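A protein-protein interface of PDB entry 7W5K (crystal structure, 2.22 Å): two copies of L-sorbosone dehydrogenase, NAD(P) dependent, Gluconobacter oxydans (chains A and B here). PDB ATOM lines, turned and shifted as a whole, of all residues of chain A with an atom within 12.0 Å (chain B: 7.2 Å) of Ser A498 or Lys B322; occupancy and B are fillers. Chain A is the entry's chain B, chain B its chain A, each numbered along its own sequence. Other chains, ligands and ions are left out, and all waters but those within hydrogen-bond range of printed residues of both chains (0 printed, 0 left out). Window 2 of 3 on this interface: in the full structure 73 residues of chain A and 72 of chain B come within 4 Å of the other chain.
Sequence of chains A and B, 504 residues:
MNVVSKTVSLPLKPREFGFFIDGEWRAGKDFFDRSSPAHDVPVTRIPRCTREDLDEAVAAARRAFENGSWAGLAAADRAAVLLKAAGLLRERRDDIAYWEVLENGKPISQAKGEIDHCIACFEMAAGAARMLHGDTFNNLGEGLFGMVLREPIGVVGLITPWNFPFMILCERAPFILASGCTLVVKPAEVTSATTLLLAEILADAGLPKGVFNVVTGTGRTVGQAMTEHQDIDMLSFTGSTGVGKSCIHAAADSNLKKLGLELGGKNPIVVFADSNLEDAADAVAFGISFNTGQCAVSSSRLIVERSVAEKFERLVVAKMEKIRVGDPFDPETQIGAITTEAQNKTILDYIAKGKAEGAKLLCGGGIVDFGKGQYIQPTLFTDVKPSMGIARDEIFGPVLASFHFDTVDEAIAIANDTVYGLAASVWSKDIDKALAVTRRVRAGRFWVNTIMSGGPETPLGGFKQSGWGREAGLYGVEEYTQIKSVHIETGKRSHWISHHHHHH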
ATOM      1  N   ARG A 493     -19.770 -24.921 -20.958  1.00  0.00           N
ATOM      2  CA  ARG A 493     -20.357 -23.616 -20.715  1.00  0.00           C
ATOM      3  C   ARG A 493     -20.469 -22.853 -22.029  1.00  0.00           C
ATOM      4  O   ARG A 493     -19.529 -22.827 -22.836  1.00  0.00           O
ATOM      5  CB  ARG A 493     -19.521 -22.850 -19.685  1.00  0.00           C
ATOM      6  CG  ARG A 493     -19.430 -21.362 -19.902  1.00  0.00           C
ATOM      7  CD  ARG A 493     -18.618 -20.678 -18.802  1.00  0.00           C
ATOM      8  NE  ARG A 493     -19.081 -19.309 -18.595  1.00  0.00           N
ATOM      9  CZ  ARG A 493     -20.116 -18.960 -17.839  1.00  0.00           C
ATOM     10  NH1 ARG A 493     -20.785 -19.856 -17.121  1.00  0.00           N
ATOM     11  NH2 ARG A 493     -20.488 -17.680 -17.803  1.00  0.00           N
ATOM     12  N   SER A 494     -21.645 -22.292 -22.275  1.00  0.00           N
ATOM     13  CA  SER A 494     -21.790 -21.363 -23.379  1.00  0.00           C
ATOM     14  C   SER A 494     -21.240 -20.029 -22.907  1.00  0.00           C
ATOM     15  O   SER A 494     -21.786 -19.431 -21.977  1.00  0.00           O
ATOM     16  CB  SER A 494     -23.244 -21.237 -23.814  1.00  0.00           C
ATOM     17  OG  SER A 494     -23.316 -20.557 -25.055  1.00  0.00           O
ATOM     18  N   HIS A 495     -20.143 -19.584 -23.519  1.00  0.00           N
ATOM     19  CA  HIS A 495     -19.409 -18.448 -22.986  1.00  0.00           C
ATOM     20  C   HIS A 495     -20.231 -17.169 -23.059  1.00  0.00           C
ATOM     21  O   HIS A 495     -20.979 -16.936 -24.016  1.00  0.00           O
ATOM     22  CB  HIS A 495     -18.089 -18.267 -23.721  1.00  0.00           C
ATOM     23  CG  HIS A 495     -17.007 -19.163 -23.217  1.00  0.00           C
ATOM     24  ND1 HIS A 495     -15.673 -18.830 -23.289  1.00  0.00           N
ATOM     25  CD2 HIS A 495     -17.061 -20.387 -22.639  1.00  0.00           C
ATOM     26  CE1 HIS A 495     -14.952 -19.808 -22.769  1.00  0.00           C
ATOM     27  NE2 HIS A 495     -15.770 -20.767 -22.373  1.00  0.00           N
ATOM     28  N   TRP A 496     -20.094 -16.349 -22.017  1.00  0.00           N
ATOM     29  CA  TRP A 496     -20.729 -15.038 -21.991  1.00  0.00           C
ATOM     30  C   TRP A 496     -19.999 -14.048 -22.885  1.00  0.00           C
ATOM     31  O   TRP A 496     -20.631 -13.169 -23.485  1.00  0.00           O
ATOM     32  CB  TRP A 496     -20.768 -14.533 -20.551  1.00  0.00           C
ATOM     33  CG  TRP A 496     -21.481 -13.233 -20.337  1.00  0.00           C
ATOM     34  CD1 TRP A 496     -22.769 -12.936 -20.660  1.00  0.00           C
ATOM     35  CD2 TRP A 496     -20.941 -12.066 -19.709  1.00  0.00           C
ATOM     36  NE1 TRP A 496     -23.061 -11.645 -20.283  1.00  0.00           N
ATOM     37  CE2 TRP A 496     -21.955 -11.093 -19.693  1.00  0.00           C
ATOM     38  CE3 TRP A 496     -19.701 -11.756 -19.154  1.00  0.00           C
ATOM     39  CZ2 TRP A 496     -21.766  -9.830 -19.143  1.00  0.00           C
ATOM     40  CZ3 TRP A 496     -19.510 -10.501 -18.612  1.00  0.00           C
ATOM     41  CH2 TRP A 496     -20.540  -9.554 -18.608  1.00  0.00           C
ATOM     42  N   ILE A 497     -18.685 -14.201 -23.007  1.00  0.00           N
ATOM     43  CA  ILE A 497     -17.828 -13.284 -23.747  1.00  0.00           C
ATOM     44  C   ILE A 497     -17.267 -14.035 -24.945  1.00  0.00           C
ATOM     45  O   ILE A 497     -16.634 -15.089 -24.787  1.00  0.00           O
ATOM     46  CB  ILE A 497     -16.699 -12.743 -22.857  1.00  0.00           C
ATOM     47  CG1 ILE A 497     -17.279 -11.971 -21.678  1.00  0.00           C
ATOM     48  CG2 ILE A 497     -15.754 -11.868 -23.652  1.00  0.00           C
ATOM     49  CD1 ILE A 497     -16.345 -11.909 -20.535  1.00  0.00           C
ATOM     50  N   SER A 498     -17.487 -13.481 -26.138  1.00  0.00           N
ATOM     51  CA  SER A 498     -17.000 -14.051 -27.396  1.00  0.00           C
ATOM     52  C   SER A 498     -15.469 -14.068 -27.473  1.00  0.00           C
ATOM     53  O   SER A 498     -14.817 -13.017 -27.494  1.00  0.00           O
ATOM     54  CB  SER A 498     -17.575 -13.267 -28.578  1.00  0.00           C
ATOM     55  OG  SER A 498     -18.829 -13.801 -28.969  1.00  0.00           O
ATOM     56  N   ASP B 282     -14.141 -17.213 -18.393  1.00  0.00           N
ATOM     57  CA  ASP B 282     -15.377 -16.581 -18.830  1.00  0.00           C
ATOM     58  C   ASP B 282     -16.338 -16.402 -17.659  1.00  0.00           C
ATOM     59  O   ASP B 282     -16.906 -15.320 -17.456  1.00  0.00           O
ATOM     60  CB  ASP B 282     -16.015 -17.417 -19.938  1.00  0.00           C
ATOM     61  CG  ASP B 282     -17.231 -16.746 -20.543  1.00  0.00           C
ATOM     62  OD1 ASP B 282     -17.059 -15.823 -21.366  1.00  0.00           O
ATOM     63  OD2 ASP B 282     -18.366 -17.148 -20.211  1.00  0.00           O
ATOM     64  N   LEU B 315      -6.103 -14.665 -18.575  1.00  0.00           N
ATOM     65  CA  LEU B 315      -7.311 -15.094 -19.277  1.00  0.00           C
ATOM     66  C   LEU B 315      -8.514 -14.240 -18.880  1.00  0.00           C
ATOM     67  O   LEU B 315      -9.326 -13.848 -19.731  1.00  0.00           O
ATOM     68  CB  LEU B 315      -7.607 -16.561 -18.978  1.00  0.00           C
ATOM     69  CG  LEU B 315      -6.969 -17.701 -19.760  1.00  0.00           C
ATOM     70  CD1 LEU B 315      -7.489 -19.007 -19.188  1.00  0.00           C
ATOM     71  CD2 LEU B 315      -7.261 -17.602 -21.251  1.00  0.00           C
ATOM     72  N   VAL B 316      -8.636 -13.937 -17.586  1.00  0.00           N
ATOM     73  CA  VAL B 316      -9.760 -13.135 -17.117  1.00  0.00           C
ATOM     74  C   VAL B 316      -9.652 -11.712 -17.642  1.00  0.00           C
ATOM     75  O   VAL B 316     -10.651 -11.118 -18.059  1.00  0.00           O
ATOM     76  CB  VAL B 316      -9.846 -13.195 -15.583  1.00  0.00           C
ATOM     77  CG1 VAL B 316     -10.933 -12.252 -15.060  1.00  0.00           C
ATOM     78  CG2 VAL B 316     -10.107 -14.644 -15.141  1.00  0.00           C
ATOM     79  N   VAL B 317      -8.446 -11.145 -17.633  1.00  0.00           N
ATOM     80  CA  VAL B 317      -8.253  -9.825 -18.222  1.00  0.00           C
ATOM     81  C   VAL B 317      -8.701  -9.833 -19.678  1.00  0.00           C
ATOM     82  O   VAL B 317      -9.475  -8.974 -20.110  1.00  0.00           O
ATOM     83  CB  VAL B 317      -6.785  -9.381 -18.092  1.00  0.00           C
ATOM     84  CG1 VAL B 317      -6.539  -8.136 -18.935  1.00  0.00           C
ATOM     85  CG2 VAL B 317      -6.420  -9.133 -16.640  1.00  0.00           C
ATOM     86  N   ALA B 318      -8.219 -10.805 -20.454  1.00  0.00           N
ATOM     87  CA  ALA B 318      -8.623 -10.897 -21.850  1.00  0.00           C
ATOM     88  C   ALA B 318     -10.131 -11.004 -21.959  1.00  0.00           C
ATOM     89  O   ALA B 318     -10.733 -10.518 -22.921  1.00  0.00           O
ATOM     90  CB  ALA B 318      -7.923 -12.062 -22.551  1.00  0.00           C
ATOM     91  N   LYS B 319     -10.759 -11.708 -21.032  1.00  0.00           N
ATOM     92  CA  LYS B 319     -12.209 -11.759 -21.095  1.00  0.00           C
ATOM     93  C   LYS B 319     -12.815 -10.394 -20.745  1.00  0.00           C
ATOM     94  O   LYS B 319     -13.786  -9.960 -21.376  1.00  0.00           O
ATOM     95  CB  LYS B 319     -12.706 -12.892 -20.204  1.00  0.00           C
ATOM     96  CG  LYS B 319     -12.710 -14.262 -20.908  1.00  0.00           C
ATOM     97  CD  LYS B 319     -14.102 -14.603 -21.421  1.00  0.00           C
ATOM     98  CE  LYS B 319     -14.132 -15.625 -22.561  1.00  0.00           C
ATOM     99  NZ  LYS B 319     -12.970 -16.537 -22.472  1.00  0.00           N
ATOM    100  N   MET B 320     -12.295  -9.748 -19.715  1.00  0.00           N
ATOM    101  CA  MET B 320     -12.891  -8.478 -19.250  1.00  0.00           C
ATOM    102  C   MET B 320     -12.759  -7.404 -20.328  1.00  0.00           C
ATOM    103  O   MET B 320     -13.684  -6.613 -20.460  1.00  0.00           O
ATOM    104  CB  MET B 320     -12.195  -8.012 -17.971  1.00  0.00           C
ATOM    105  CG  MET B 320     -12.577  -8.793 -16.738  1.00  0.00           C
ATOM    106  SD  MET B 320     -11.666  -8.158 -15.320  1.00  0.00           S
ATOM    107  CE  MET B 320     -12.740  -8.648 -13.975  1.00  0.00           C
ATOM    108  N   GLU B 321     -11.657  -7.425 -21.067  1.00  0.00           N
ATOM    109  CA  GLU B 321     -11.367  -6.405 -22.095  1.00  0.00           C
ATOM    110  C   GLU B 321     -12.376  -6.497 -23.231  1.00  0.00           C
ATOM    111  O   GLU B 321     -12.591  -5.489 -23.898  1.00  0.00           O
ATOM    112  CB  GLU B 321      -9.960  -6.647 -22.626  1.00  0.00           C
ATOM    113  CG  GLU B 321      -8.994  -5.519 -22.321  1.00  0.00           C
ATOM    114  CD  GLU B 321      -8.649  -5.335 -20.854  1.00  0.00           C
ATOM    115  OE1 GLU B 321      -8.952  -6.237 -20.055  1.00  0.00           O
ATOM    116  OE2 GLU B 321      -8.076  -4.287 -20.517  1.00  0.00           O
ATOM    117  N   LYS B 322     -12.975  -7.669 -23.415  1.00  0.00           N
ATOM    118  CA  LYS B 322     -13.980  -7.788 -24.458  1.00  0.00           C
ATOM    119  C   LYS B 322     -15.394  -7.658 -23.956  1.00  0.00           C
ATOM    120  O   LYS B 322     -16.311  -7.858 -24.739  1.00  0.00           O
ATOM    121  CB  LYS B 322     -13.791  -9.110 -25.188  1.00  0.00           C
ATOM    122  CG  LYS B 322     -12.350  -9.410 -25.506  1.00  0.00           C
ATOM    123  CD  LYS B 322     -12.178 -10.168 -26.792  1.00  0.00           C
ATOM    124  CE  LYS B 322     -11.984 -11.665 -26.524  1.00  0.00           C
ATOM    125  NZ  LYS B 322     -10.594 -11.946 -26.048  1.00  0.00           N
ATOM    126  N   ILE B 323     -15.602  -7.394 -22.670  1.00  0.00           N
ATOM    127  CA  ILE B 323     -16.969  -7.222 -22.201  1.00  0.00           C
ATOM    128  C   ILE B 323     -17.530  -5.951 -22.823  1.00  0.00           C
ATOM    129  O   ILE B 323     -16.955  -4.867 -22.681  1.00  0.00           O
ATOM    130  CB  ILE B 323     -17.030  -7.171 -20.675  1.00  0.00           C
ATOM    131  CG1 ILE B 323     -16.844  -8.571 -20.111  1.00  0.00           C
ATOM    132  CG2 ILE B 323     -18.335  -6.580 -20.223  1.00  0.00           C
ATOM    133  CD1 ILE B 323     -16.418  -8.564 -18.690  1.00  0.00           C
ATOM    134  N   ARG B 324     -18.639  -6.085 -23.544  1.00  0.00           N
ATOM    135  CA  ARG B 324     -19.226  -4.935 -24.222  1.00  0.00           C
ATOM    136  C   ARG B 324     -19.874  -4.023 -23.187  1.00  0.00           C
ATOM    137  O   ARG B 324     -20.906  -4.361 -22.597  1.00  0.00           O
ATOM    138  CB  ARG B 324     -20.216  -5.399 -25.286  1.00  0.00           C
ATOM    139  CG  ARG B 324     -19.513  -6.053 -26.479  1.00  0.00           C
ATOM    140  CD  ARG B 324     -20.468  -6.593 -27.563  1.00  0.00           C
ATOM    141  NE  ARG B 324     -21.479  -7.522 -27.060  1.00  0.00           N
ATOM    142  CZ  ARG B 324     -21.336  -8.840 -26.979  1.00  0.00           C
ATOM    143  NH1 ARG B 324     -20.221  -9.442 -27.366  1.00  0.00           N
ATOM    144  NH2 ARG B 324     -22.347  -9.577 -26.512  1.00  0.00           N
ATOM    145  N   VAL B 325     -19.226  -2.888 -22.932  1.00  0.00           N
ATOM    146  CA  VAL B 325     -19.761  -1.825 -22.094  1.00  0.00           C
ATOM    147  C   VAL B 325     -20.391  -0.797 -23.013  1.00  0.00           C
ATOM    148  O   VAL B 325     -19.864  -0.514 -24.094  1.00  0.00           O
ATOM    149  CB  VAL B 325     -18.662  -1.179 -21.224  1.00  0.00           C
ATOM    150  CG1 VAL B 325     -19.288  -0.330 -20.115  1.00  0.00           C
ATOM    151  CG2 VAL B 325     -17.751  -2.231 -20.631  1.00  0.00           C
ATOM    152  N   GLN B 334     -23.207  -5.663 -22.758  1.00  0.00           N
ATOM    153  CA  GLN B 334     -23.195  -6.734 -21.778  1.00  0.00           C
ATOM    154  C   GLN B 334     -23.191  -6.233 -20.341  1.00  0.00           C
ATOM    155  O   GLN B 334     -23.745  -6.901 -19.460  1.00  0.00           O
ATOM    156  CB  GLN B 334     -21.991  -7.641 -22.013  1.00  0.00           C
ATOM    157  CG  GLN B 334     -22.034  -8.355 -23.344  1.00  0.00           C
ATOM    158  CD  GLN B 334     -20.894  -9.354 -23.502  1.00  0.00           C
ATOM    159  OE1 GLN B 334     -19.723  -8.974 -23.549  1.00  0.00           O
ATOM    160  NE2 GLN B 334     -21.233 -10.636 -23.562  1.00  0.00           N
ATOM    161  N   PRO B 378     -14.624  -3.307 -16.204  1.00  0.00           N
ATOM    162  CA  PRO B 378     -14.337  -4.522 -15.440  1.00  0.00           C
ATOM    163  C   PRO B 378     -12.886  -4.516 -14.990  1.00  0.00           C
ATOM    164  O   PRO B 378     -11.965  -4.333 -15.789  1.00  0.00           O
ATOM    165  CB  PRO B 378     -14.636  -5.641 -16.435  1.00  0.00           C
ATOM    166  CG  PRO B 378     -15.708  -5.053 -17.306  1.00  0.00           C
ATOM    167  CD  PRO B 378     -15.348  -3.597 -17.450  1.00  0.00           C
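The side-chain amide nitrogen (NE2) of Gln B334 is in hydrogen-bond range of the backbone carbonyl oxygen (O) of Trp A496, 2.6 Å away. OD2 of Asp B282 lies within salt-bridge range of NE of Arg A493. The backbone NH (N) of Ile A497 is in hydrogen-bond range of the side-chain carboxylate (OD1) of Asp B282 (2.8 Å). The backbone NH of Trp A496 is in hydrogen-bond range of the side-chain carboxylate of Asp B282, at 2.6 Å.
The backbone NH of Gln B334 is in hydrogen-bond range of the backbone carbonyl oxygen of Arg B324 (2.6 Å). O of Ala B318 sits close to NZ of Lys B322, 3.4 Å away.
Among the printed residues, pairs that only touch across the chains: His A495 with Asp B282, Ser A498 with Lys B322, Ile A497 with Lys B319, Ile A497 with Ile B323, Trp A496 with Ile B323, His A495 with Lys B319 and Ile A497 with Lys B322.
Of the printed residues of chain B, Ser A498 touches Lys B322. Lys B322 touches just these residues of chain A: Ile A497 (3.7 Å) and Ser A498 (3.3 Å). No residue of chain A comes within 4 Å of Ala B318. No residue of chain A comes within 4 Å of Glu B321. Ile B323 touches just these residues of chain A: Trp A496 (3.6 Å) and Ile A497 (3.4 Å). No residue of chain A comes within 4 Å of Arg B324. Of the printed residues of chain B, His A495 touches Asp B282 and Lys B319. Of the printed residues of chain B, Trp A496 touches Asp B282 (2.6 Å), Ile B323 (3.6 Å) and Gln B334 (2.6 Å). Val B316 touches none of the printed residues of chain A. Met B320 touches none of the printed residues of chain A. The nearest residue of chain B that does not touch Ser A498 is Arg B324 (4.8 Å). The nearest residue of chain A that does not touch Lys B322 is Trp A496 (7.0 Å). The nearest printed residue of chain B that does not touch Ile A497 is Gln B334 (4.3 Å).
Hydrophobic or aromatic side chains of chain B that line the printed part of chain A: Ile B323. Of the 6 printed residues of chain A, 5 touch a printed residue of chain B. Among the printed residues, 11 pairs touch across the chains. Among the printed residues, Asp or Glu carboxylates within 4 Å of a Lys or Arg side-chain nitrogen of the other chain: Arg A493 with Asp B282 (2.8 Å).
No position is printed for both chains. Of the 11 pairs that touch across the chains among the printed residues, none has its exchanged pair printed and touching as well.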
